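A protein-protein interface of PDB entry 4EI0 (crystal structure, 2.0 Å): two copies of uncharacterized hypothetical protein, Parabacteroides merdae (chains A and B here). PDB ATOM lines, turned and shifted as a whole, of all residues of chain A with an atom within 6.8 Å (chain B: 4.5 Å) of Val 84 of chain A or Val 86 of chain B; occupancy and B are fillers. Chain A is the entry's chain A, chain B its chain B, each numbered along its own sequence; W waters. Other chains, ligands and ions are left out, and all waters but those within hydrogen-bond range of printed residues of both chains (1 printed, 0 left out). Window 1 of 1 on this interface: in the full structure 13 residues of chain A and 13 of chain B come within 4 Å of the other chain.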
ATOM      1  N   PRO A  70     -27.749 -24.933   1.189  1.00  0.00           N
ATOM      2  CA  PRO A  70     -27.732 -23.504   1.011  1.00  0.00           C
ATOM      3  C   PRO A  70     -26.554 -22.973   0.185  1.00  0.00           C
ATOM      4  O   PRO A  70     -26.459 -21.753  -0.002  1.00  0.00           O
ATOM      5  CB  PRO A  70     -27.672 -22.982   2.443  1.00  0.00           C
ATOM      6  CG  PRO A  70     -26.941 -24.054   3.206  1.00  0.00           C
ATOM      7  CD  PRO A  70     -27.307 -25.343   2.537  1.00  0.00           C
ATOM      8  N   ASN A  71     -25.642 -23.834  -0.280  1.00  0.00           N
ATOM      9  CA  ASN A  71     -24.543 -23.347  -1.084  1.00  0.00           C
ATOM     10  C   ASN A  71     -24.870 -23.444  -2.569  1.00  0.00           C
ATOM     11  O   ASN A  71     -25.379 -24.434  -3.012  1.00  0.00           O
ATOM     12  CB  ASN A  71     -23.291 -24.144  -0.853  1.00  0.00           C
ATOM     13  CG  ASN A  71     -22.792 -24.034   0.545  1.00  0.00           C
ATOM     14  OD1 ASN A  71     -22.140 -23.052   0.919  1.00  0.00           O
ATOM     15  ND2 ASN A  71     -23.069 -25.090   1.336  1.00  0.00           N
ATOM     16  N   SER A  72     -24.530 -22.419  -3.332  1.00  0.00           N
ATOM     17  CA  SER A  72     -24.518 -22.551  -4.758  1.00  0.00           C
ATOM     18  C   SER A  72     -23.161 -23.131  -5.135  1.00  0.00           C
ATOM     19  O   SER A  72     -22.132 -22.766  -4.582  1.00  0.00           O
ATOM     20  CB  SER A  72     -24.745 -21.217  -5.480  1.00  0.00           C
ATOM     21  OG  SER A  72     -24.501 -21.371  -6.881  1.00  0.00           O
ATOM     22  N   TYR A  73     -23.173 -24.085  -6.057  1.00  0.00           N
ATOM     23  CA  TYR A  73     -21.956 -24.769  -6.494  1.00  0.00           C
ATOM     24  C   TYR A  73     -21.571 -24.197  -7.819  1.00  0.00           C
ATOM     25  O   TYR A  73     -22.225 -24.495  -8.793  1.00  0.00           O
ATOM     26  CB  TYR A  73     -22.226 -26.292  -6.573  1.00  0.00           C
ATOM     27  CG  TYR A  73     -22.309 -26.863  -5.176  1.00  0.00           C
ATOM     28  CD1 TYR A  73     -21.159 -27.254  -4.496  1.00  0.00           C
ATOM     29  CD2 TYR A  73     -23.505 -26.914  -4.509  1.00  0.00           C
ATOM     30  CE1 TYR A  73     -21.215 -27.724  -3.201  1.00  0.00           C
ATOM     31  CE2 TYR A  73     -23.568 -27.344  -3.202  1.00  0.00           C
ATOM     32  CZ  TYR A  73     -22.409 -27.750  -2.567  1.00  0.00           C
ATOM     33  OH  TYR A  73     -22.474 -28.137  -1.269  1.00  0.00           O
ATOM     34  N   TYR A  74     -20.535 -23.376  -7.855  1.00  0.00           N
ATOM     35  CA  TYR A  74     -19.926 -22.832  -9.083  1.00  0.00           C
ATOM     36  C   TYR A  74     -18.751 -23.775  -9.461  1.00  0.00           C
ATOM     37  O   TYR A  74     -18.356 -24.607  -8.658  1.00  0.00           O
ATOM     38  CB  TYR A  74     -19.474 -21.366  -8.876  1.00  0.00           C
ATOM     39  CG  TYR A  74     -20.637 -20.458  -8.512  1.00  0.00           C
ATOM     40  CD1 TYR A  74     -21.556 -20.070  -9.454  1.00  0.00           C
ATOM     41  CD2 TYR A  74     -20.869 -20.105  -7.194  1.00  0.00           C
ATOM     42  CE1 TYR A  74     -22.647 -19.295  -9.097  1.00  0.00           C
ATOM     43  CE2 TYR A  74     -21.973 -19.326  -6.826  1.00  0.00           C
ATOM     44  CZ  TYR A  74     -22.840 -18.908  -7.786  1.00  0.00           C
ATOM     45  OH  TYR A  74     -23.935 -18.162  -7.430  1.00  0.00           O
ATOM     46  N   ILE A  82     -17.017 -25.083  -6.447  1.00  0.00           N
ATOM     47  CA  ILE A  82     -16.740 -24.028  -5.448  1.00  0.00           C
ATOM     48  C   ILE A  82     -18.070 -23.742  -4.760  1.00  0.00           C
ATOM     49  O   ILE A  82     -18.957 -23.158  -5.385  1.00  0.00           O
ATOM     50  CB  ILE A  82     -16.212 -22.725  -6.048  1.00  0.00           C
ATOM     51  CG1 ILE A  82     -14.983 -22.967  -6.935  1.00  0.00           C
ATOM     52  CG2 ILE A  82     -15.882 -21.747  -4.931  1.00  0.00           C
ATOM     53  CD1 ILE A  82     -14.697 -21.830  -7.914  1.00  0.00           C
ATOM     54  N   PRO A  83     -18.237 -24.209  -3.511  1.00  0.00           N
ATOM     55  CA  PRO A  83     -19.491 -23.912  -2.807  1.00  0.00           C
ATOM     56  C   PRO A  83     -19.391 -22.495  -2.234  1.00  0.00           C
ATOM     57  O   PRO A  83     -18.311 -22.083  -1.752  1.00  0.00           O
ATOM     58  CB  PRO A  83     -19.548 -24.948  -1.692  1.00  0.00           C
ATOM     59  CG  PRO A  83     -18.151 -25.368  -1.477  1.00  0.00           C
ATOM     60  CD  PRO A  83     -17.413 -25.184  -2.768  1.00  0.00           C
ATOM     61  N   VAL A  84     -20.460 -21.737  -2.452  1.00  0.00           N
ATOM     62  CA  VAL A  84     -20.583 -20.360  -1.981  1.00  0.00           C
ATOM     63  C   VAL A  84     -21.939 -20.291  -1.241  1.00  0.00           C
ATOM     64  O   VAL A  84     -22.995 -20.617  -1.805  1.00  0.00           O
ATOM     65  CB  VAL A  84     -20.511 -19.346  -3.098  1.00  0.00           C
ATOM     66  CG1 VAL A  84     -20.600 -17.943  -2.506  1.00  0.00           C
ATOM     67  CG2 VAL A  84     -19.198 -19.518  -3.840  1.00  0.00           C
ATOM     68  N   LYS A  85     -21.902 -19.861   0.011  1.00  0.00           N
ATOM     69  CA  LYS A  85     -23.081 -19.934   0.871  1.00  0.00           C
ATOM     70  C   LYS A  85     -23.977 -18.731   0.613  1.00  0.00           C
ATOM     71  O   LYS A  85     -23.822 -17.681   1.213  1.00  0.00           O
ATOM     72  CB  LYS A  85     -22.613 -20.004   2.323  1.00  0.00           C
ATOM     73  CG  LYS A  85     -23.677 -19.955   3.399  1.00  0.00           C
ATOM     74  CD  LYS A  85     -24.276 -21.265   3.708  1.00  0.00           C
ATOM     75  CE  LYS A  85     -25.231 -21.127   4.890  1.00  0.00           C
ATOM     76  NZ  LYS A  85     -24.729 -22.030   5.947  1.00  0.00           N
ATOM     77  N   VAL A  86     -24.881 -18.892  -0.332  1.00  0.00           N
ATOM     78  CA  VAL A  86     -25.647 -17.777  -0.840  1.00  0.00           C
ATOM     79  C   VAL A  86     -27.085 -17.751  -0.286  1.00  0.00           C
ATOM     80  O   VAL A  86     -27.754 -16.755  -0.435  1.00  0.00           O
ATOM     81  CB  VAL A  86     -25.694 -17.715  -2.394  1.00  0.00           C
ATOM     82  CG1 VAL A  86     -24.323 -17.355  -2.946  1.00  0.00           C
ATOM     83  CG2 VAL A  86     -26.402 -18.948  -2.986  1.00  0.00           C
ATOM     84  N   CYS A  87     -27.512 -18.797   0.409  1.00  0.00           N
ATOM     85  CA  CYS A  87     -28.856 -18.858   0.955  1.00  0.00           C
ATOM     86  C   CYS A  87     -28.858 -19.068   2.468  1.00  0.00           C
ATOM     87  O   CYS A  87     -27.890 -19.543   3.056  1.00  0.00           O
ATOM     88  CB  CYS A  87     -29.583 -20.038   0.378  1.00  0.00           C
ATOM     89  SG  CYS A  87     -29.867 -19.975  -1.384  1.00  0.00           S
ATOM     90  N   VAL A 103     -27.603 -13.603  -0.294  1.00  0.00           N
ATOM     91  CA  VAL A 103     -26.466 -12.971  -0.959  1.00  0.00           C
ATOM     92  C   VAL A 103     -26.884 -12.596  -2.401  1.00  0.00           C
ATOM     93  O   VAL A 103     -27.583 -13.371  -3.075  1.00  0.00           O
ATOM     94  CB  VAL A 103     -25.291 -13.968  -0.989  1.00  0.00           C
ATOM     95  CG1 VAL A 103     -24.109 -13.441  -1.802  1.00  0.00           C
ATOM     96  CG2 VAL A 103     -24.883 -14.375   0.433  1.00  0.00           C
ATOM     97  N   ASP A 104     -26.510 -11.424  -2.875  1.00  0.00           N
ATOM     98  CA  ASP A 104     -26.881 -11.022  -4.262  1.00  0.00           C
ATOM     99  C   ASP A 104     -26.079 -11.851  -5.284  1.00  0.00           C
ATOM    100  O   ASP A 104     -24.825 -11.858  -5.280  1.00  0.00           O
ATOM    101  CB  ASP A 104     -26.584  -9.569  -4.545  1.00  0.00           C
ATOM    102  CG  ASP A 104     -27.647  -8.597  -4.020  1.00  0.00           C
ATOM    103  OD1 ASP A 104     -28.654  -9.029  -3.421  1.00  0.00           O
ATOM    104  OD2 ASP A 104     -27.408  -7.366  -4.186  1.00  0.00           O
ATOM    105  N   LEU A 110     -28.302 -24.813  -7.074  1.00  0.00           N
ATOM    106  CA  LEU A 110     -28.548 -25.348  -5.733  1.00  0.00           C
ATOM    107  C   LEU A 110     -28.886 -26.821  -5.879  1.00  0.00           C
ATOM    108  O   LEU A 110     -29.502 -27.225  -6.886  1.00  0.00           O
ATOM    109  CB  LEU A 110     -29.728 -24.657  -5.101  1.00  0.00           C
ATOM    110  CG  LEU A 110     -29.616 -23.168  -4.797  1.00  0.00           C
ATOM    111  CD1 LEU A 110     -30.948 -22.738  -4.214  1.00  0.00           C
ATOM    112  CD2 LEU A 110     -28.452 -22.893  -3.843  1.00  0.00           C
ATOM    113  N   PRO B  70     -16.737  -5.655  -4.716  1.00  0.00           N
ATOM    114  CA  PRO B  70     -17.039  -6.640  -3.696  1.00  0.00           C
ATOM    115  C   PRO B  70     -17.583  -7.964  -4.258  1.00  0.00           C
ATOM    116  O   PRO B  70     -17.949  -8.857  -3.457  1.00  0.00           O
ATOM    117  CB  PRO B  70     -18.092  -5.924  -2.814  1.00  0.00           C
ATOM    118  CG  PRO B  70     -18.806  -5.009  -3.779  1.00  0.00           C
ATOM    119  CD  PRO B  70     -17.782  -4.595  -4.796  1.00  0.00           C
ATOM    120  N   SER B  72     -17.277 -11.531  -6.250  1.00  0.00           N
ATOM    121  CA  SER B  72     -16.394 -12.497  -6.850  1.00  0.00           C
ATOM    122  C   SER B  72     -17.011 -12.855  -8.178  1.00  0.00           C
ATOM    123  O   SER B  72     -18.203 -13.021  -8.285  1.00  0.00           O
ATOM    124  CB  SER B  72     -16.208 -13.743  -5.987  1.00  0.00           C
ATOM    125  OG  SER B  72     -15.575 -14.765  -6.728  1.00  0.00           O
ATOM    126  N   TYR B  74     -17.242 -15.581 -10.795  1.00  0.00           N
ATOM    127  CA  TYR B  74     -17.139 -16.980 -11.138  1.00  0.00           C
ATOM    128  C   TYR B  74     -17.487 -17.079 -12.656  1.00  0.00           C
ATOM    129  O   TYR B  74     -18.018 -16.142 -13.230  1.00  0.00           O
ATOM    130  CB  TYR B  74     -18.091 -17.845 -10.236  1.00  0.00           C
ATOM    131  CG  TYR B  74     -17.746 -17.735  -8.755  1.00  0.00           C
ATOM    132  CD1 TYR B  74     -16.612 -18.361  -8.240  1.00  0.00           C
ATOM    133  CD2 TYR B  74     -18.489 -16.945  -7.911  1.00  0.00           C
ATOM    134  CE1 TYR B  74     -16.262 -18.237  -6.913  1.00  0.00           C
ATOM    135  CE2 TYR B  74     -18.141 -16.812  -6.580  1.00  0.00           C
ATOM    136  CZ  TYR B  74     -17.041 -17.485  -6.086  1.00  0.00           C
ATOM    137  OH  TYR B  74     -16.639 -17.242  -4.788  1.00  0.00           O
ATOM    138  N   VAL B  84     -21.051 -12.624  -7.723  1.00  0.00           N
ATOM    139  CA  VAL B  84     -21.683 -13.033  -6.469  1.00  0.00           C
ATOM    140  C   VAL B  84     -21.120 -12.107  -5.411  1.00  0.00           C
ATOM    141  O   VAL B  84     -19.885 -11.977  -5.235  1.00  0.00           O
ATOM    142  CB  VAL B  84     -21.388 -14.518  -6.114  1.00  0.00           C
ATOM    143  CG1 VAL B  84     -22.031 -14.869  -4.757  1.00  0.00           C
ATOM    144  CG2 VAL B  84     -21.836 -15.424  -7.234  1.00  0.00           C
ATOM    145  N   LYS B  85     -21.983 -11.429  -4.692  1.00  0.00           N
ATOM    146  CA  LYS B  85     -21.518 -10.342  -3.755  1.00  0.00           C
ATOM    147  C   LYS B  85     -21.096 -10.973  -2.439  1.00  0.00           C
ATOM    148  O   LYS B  85     -21.879 -11.156  -1.527  1.00  0.00           O
ATOM    149  CB  LYS B  85     -22.605  -9.266  -3.544  1.00  0.00           C
ATOM    150  CG  LYS B  85     -22.194  -8.069  -2.662  1.00  0.00           C
ATOM    151  CD  LYS B  85     -22.658  -6.717  -3.192  1.00  0.00           C
ATOM    152  CE  LYS B  85     -22.530  -5.598  -2.143  1.00  0.00           C
ATOM    153  NZ  LYS B  85     -23.706  -4.676  -2.057  1.00  0.00           N
ATOM    154  N   VAL B  86     -19.807 -11.272  -2.340  1.00  0.00           N
ATOM    155  CA  VAL B  86     -19.284 -12.066  -1.236  1.00  0.00           C
ATOM    156  C   VAL B  86     -18.556 -11.234  -0.199  1.00  0.00           C
ATOM    157  O   VAL B  86     -18.192 -11.738   0.858  1.00  0.00           O
ATOM    158  CB  VAL B  86     -18.350 -13.184  -1.741  1.00  0.00           C
ATOM    159  CG1 VAL B  86     -19.119 -14.235  -2.576  1.00  0.00           C
ATOM    160  CG2 VAL B  86     -17.211 -12.599  -2.518  1.00  0.00           C
ATOM    161  N   CYS B  87     -18.355  -9.967  -0.487  1.00  0.00           N
ATOM    162  CA  CYS B  87     -17.628  -9.064   0.399  1.00  0.00           C
ATOM    163  C   CYS B  87     -18.418  -7.858   0.778  1.00  0.00           C
ATOM    164  O   CYS B  87     -19.378  -7.448   0.082  1.00  0.00           O
ATOM    165  CB  CYS B  87     -16.358  -8.549  -0.277  1.00  0.00           C
ATOM    166  SG  CYS B  87     -15.095  -9.747  -0.690  1.00  0.00           S
ATOM    167  N   ASP B 100     -13.195  -7.288   3.228  1.00  0.00           N
ATOM    168  CA  ASP B 100     -13.546  -8.442   4.082  1.00  0.00           C
ATOM    169  C   ASP B 100     -14.579  -9.297   3.415  1.00  0.00           C
ATOM    170  O   ASP B 100     -15.573  -8.763   2.891  1.00  0.00           O
ATOM    171  CB  ASP B 100     -14.164  -7.983   5.398  1.00  0.00           C
ATOM    172  CG  ASP B 100     -13.148  -7.432   6.368  1.00  0.00           C
ATOM    173  OD1 ASP B 100     -12.008  -7.877   6.334  1.00  0.00           O
ATOM    174  OD2 ASP B 100     -13.495  -6.554   7.166  1.00  0.00           O
ATOM    175  N   PHE B 101     -14.403 -10.620   3.493  1.00  0.00           N
ATOM    176  CA  PHE B 101     -15.453 -11.498   3.017  1.00  0.00           C
ATOM    177  C   PHE B 101     -16.557 -11.568   4.080  1.00  0.00           C
ATOM    178  O   PHE B 101     -16.276 -11.715   5.240  1.00  0.00           O
ATOM    179  CB  PHE B 101     -14.892 -12.878   2.730  1.00  0.00           C
ATOM    180  CG  PHE B 101     -14.058 -12.942   1.496  1.00  0.00           C
ATOM    181  CD1 PHE B 101     -12.743 -12.582   1.532  1.00  0.00           C
ATOM    182  CD2 PHE B 101     -14.587 -13.429   0.322  1.00  0.00           C
ATOM    183  CE1 PHE B 101     -11.976 -12.639   0.411  1.00  0.00           C
ATOM    184  CE2 PHE B 101     -13.836 -13.461  -0.820  1.00  0.00           C
ATOM    185  CZ  PHE B 101     -12.528 -13.084  -0.781  1.00  0.00           C
ATOM    186  N   THR B 102     -17.810 -11.454   3.682  1.00  0.00           N
ATOM    187  CA  THR B 102     -18.938 -11.637   4.604  1.00  0.00           C
ATOM    188  C   THR B 102     -19.706 -12.891   4.219  1.00  0.00           C
ATOM    189  O   THR B 102     -20.690 -13.183   4.833  1.00  0.00           O
ATOM    190  CB  THR B 102     -19.872 -10.407   4.581  1.00  0.00           C
ATOM    191  OG1 THR B 102     -20.149 -10.089   3.210  1.00  0.00           O
ATOM    192  CG2 THR B 102     -19.150  -9.185   5.245  1.00  0.00           C
ATOM    193  N   VAL B 103     -19.279 -13.626   3.187  1.00  0.00           N
ATOM    194  CA  VAL B 103     -19.967 -14.852   2.727  1.00  0.00           C
ATOM    195  C   VAL B 103     -18.962 -15.974   2.796  1.00  0.00           C
ATOM    196  O   VAL B 103     -17.758 -15.787   2.439  1.00  0.00           O
ATOM    197  CB  VAL B 103     -20.560 -14.683   1.305  1.00  0.00           C
ATOM    198  CG1 VAL B 103     -21.086 -16.016   0.711  1.00  0.00           C
ATOM    199  CG2 VAL B 103     -21.697 -13.629   1.293  1.00  0.00           C
ATOM    200  N   ASP B 104     -19.404 -17.157   3.222  1.00  0.00           N
ATOM    201  CA  ASP B 104     -18.480 -18.288   3.283  1.00  0.00           C
ATOM    202  C   ASP B 104     -18.184 -18.742   1.839  1.00  0.00           C
ATOM    203  O   ASP B 104     -19.109 -19.155   1.082  1.00  0.00           O
ATOM    204  CB  ASP B 104     -19.064 -19.513   3.997  1.00  0.00           C
ATOM    205  CG  ASP B 104     -19.124 -19.351   5.500  1.00  0.00           C
ATOM    206  OD1 ASP B 104     -18.657 -18.312   6.023  1.00  0.00           O
ATOM    207  OD2 ASP B 104     -19.646 -20.296   6.153  1.00  0.00           O
ATOM    208  N   THR B 105     -16.898 -18.734   1.505  1.00  0.00           N
ATOM    209  CA  THR B 105     -16.464 -19.389   0.304  1.00  0.00           C
ATOM    210  C   THR B 105     -15.044 -19.847   0.419  1.00  0.00           C
ATOM    211  O   THR B 105     -14.232 -19.236   1.113  1.00  0.00           O
ATOM    212  CB  THR B 105     -16.626 -18.473  -0.919  1.00  0.00           C
ATOM    213  OG1 THR B 105     -16.313 -19.234  -2.089  1.00  0.00           O
ATOM    214  CG2 THR B 105     -15.771 -17.254  -0.774  1.00  0.00           C
HETATM  215  O   HOH W   1     -22.188 -17.230   4.123  1.00  0.00           O
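Printed residues of chain A that touch a printed residue of chain B: Tyr 74, Ile 82, Pro 83, Val 84, Lys 85, Val 86, Val 103 and Asp 104. Among the printed residues, no Asp or Glu carboxylate lies within 4 Å of a Lys or Arg side-chain nitrogen of the other chain.
Printed residues of chain A within 4 Å of Val 86 of chain B: Val 84. Of the printed residues of chain B, Tyr 74 of chain A touches Tyr 74 and Val 84. Of the printed residues of chain A, Thr 105 of chain B touches Ile 82 (3.8 Å), Pro 83 (3.5 Å) and Val 84 (3.4 Å). Of the printed residues of chain A, Val 103 of chain B touches Val 84, Lys 85 and Val 103. Of the printed residues of chain A, Tyr 74 of chain B touches Tyr 74, Ile 82 and Val 84. Thr 102 of chain B touches none of the printed residues of chain A. Tyr 73 of chain A touches none of the printed residues of chain B.
N of Lys 85 of chain A sits close to OD1 of Asn 71 of chain A (3.3 Å). The side-chain hydroxyl (OG) of Ser 72 of chain A lies close to the side-chain hydroxyl (OH) of Tyr 74 of chain A. The backbone NH (N) of Val 103 of chain B is in hydrogen-bond range of the backbone carbonyl oxygen (O) of Val 86 of chain B. The backbone NH (N) of Ser 72 of chain A lies within hydrogen-bond range of the backbone carbonyl oxygen (O) of Val 84 of chain A (2.8 Å). The backbone carbonyl oxygen (O) of Val 84 of chain B sits at hydrogen-bond distance from the backbone NH (N) of Ser 72 of chain B. The backbone carbonyl oxygen of Pro 70 of chain B lies within hydrogen-bond range of the backbone NH of Val 86 of chain B, 3.2 Å away.
Tyr 74 of chain A touches its own counterpart, Tyr 74 of chain B. Val 84 of chain A touches Val 86 of chain B, and with the chains exchanged Val 86 of chain A touches Val 84 of chain B. Val 84 of chain A touches Asp 104 of chain B, and with the chains exchanged Asp 104 of chain A touches Val 84 of chain B. Lys 85 of chain A touches Val 103 of chain B, and with the chains exchanged Val 103 of chain A touches Lys 85 of chain B. Of the 18 pairs that touch across the chains among the printed residues, 14 have their exchanged pair printed and touching as well.
O of Asp 104 of chain B sits at hydrogen-bond distance from N of Lys 85 of chain A (3.1 Å). N of Lys 85 of chain B is in hydrogen-bond range of O of Asp 104 of chain A, 2.9 Å away. The backbone carbonyl oxygen (O) of Pro 83 of chain A lies within hydrogen-bond range of the side-chain hydroxyl (OG1) of Thr 105 of chain B (3.5 Å).
Water W1 lies within hydrogen-bond range of the backbone NH (N) of Asp 104 of chain B (2.9 Å) and the backbone carbonyl oxygen (O) of Lys 85 of chain A (3.4 Å).
Ile 82 of chain A touches Tyr 74 of chain B. CG2 of Val 84 of chain A touches OH of Tyr 74 of chain B, 3.6 Å away. Val 86 of chain B touches Val 84 of chain A (CG1 to CG1, 3.99 Å). Val 84 of chain A touches Val 103 of chain B (CG1 to CG1, 3.8 Å). CA of Val 84 of chain A touches O of Asp 104 of chain B (3.6 Å). Val 84 of chain A touches Thr 105 of chain B. Val 103 of chain B touches Lys 85 of chain A. Val 103 of chain A touches Val 84 of chain B. Val 103 of chain A touches Lys 85 of chain B. Asp 104 of chain A touches Val 84 of chain B.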
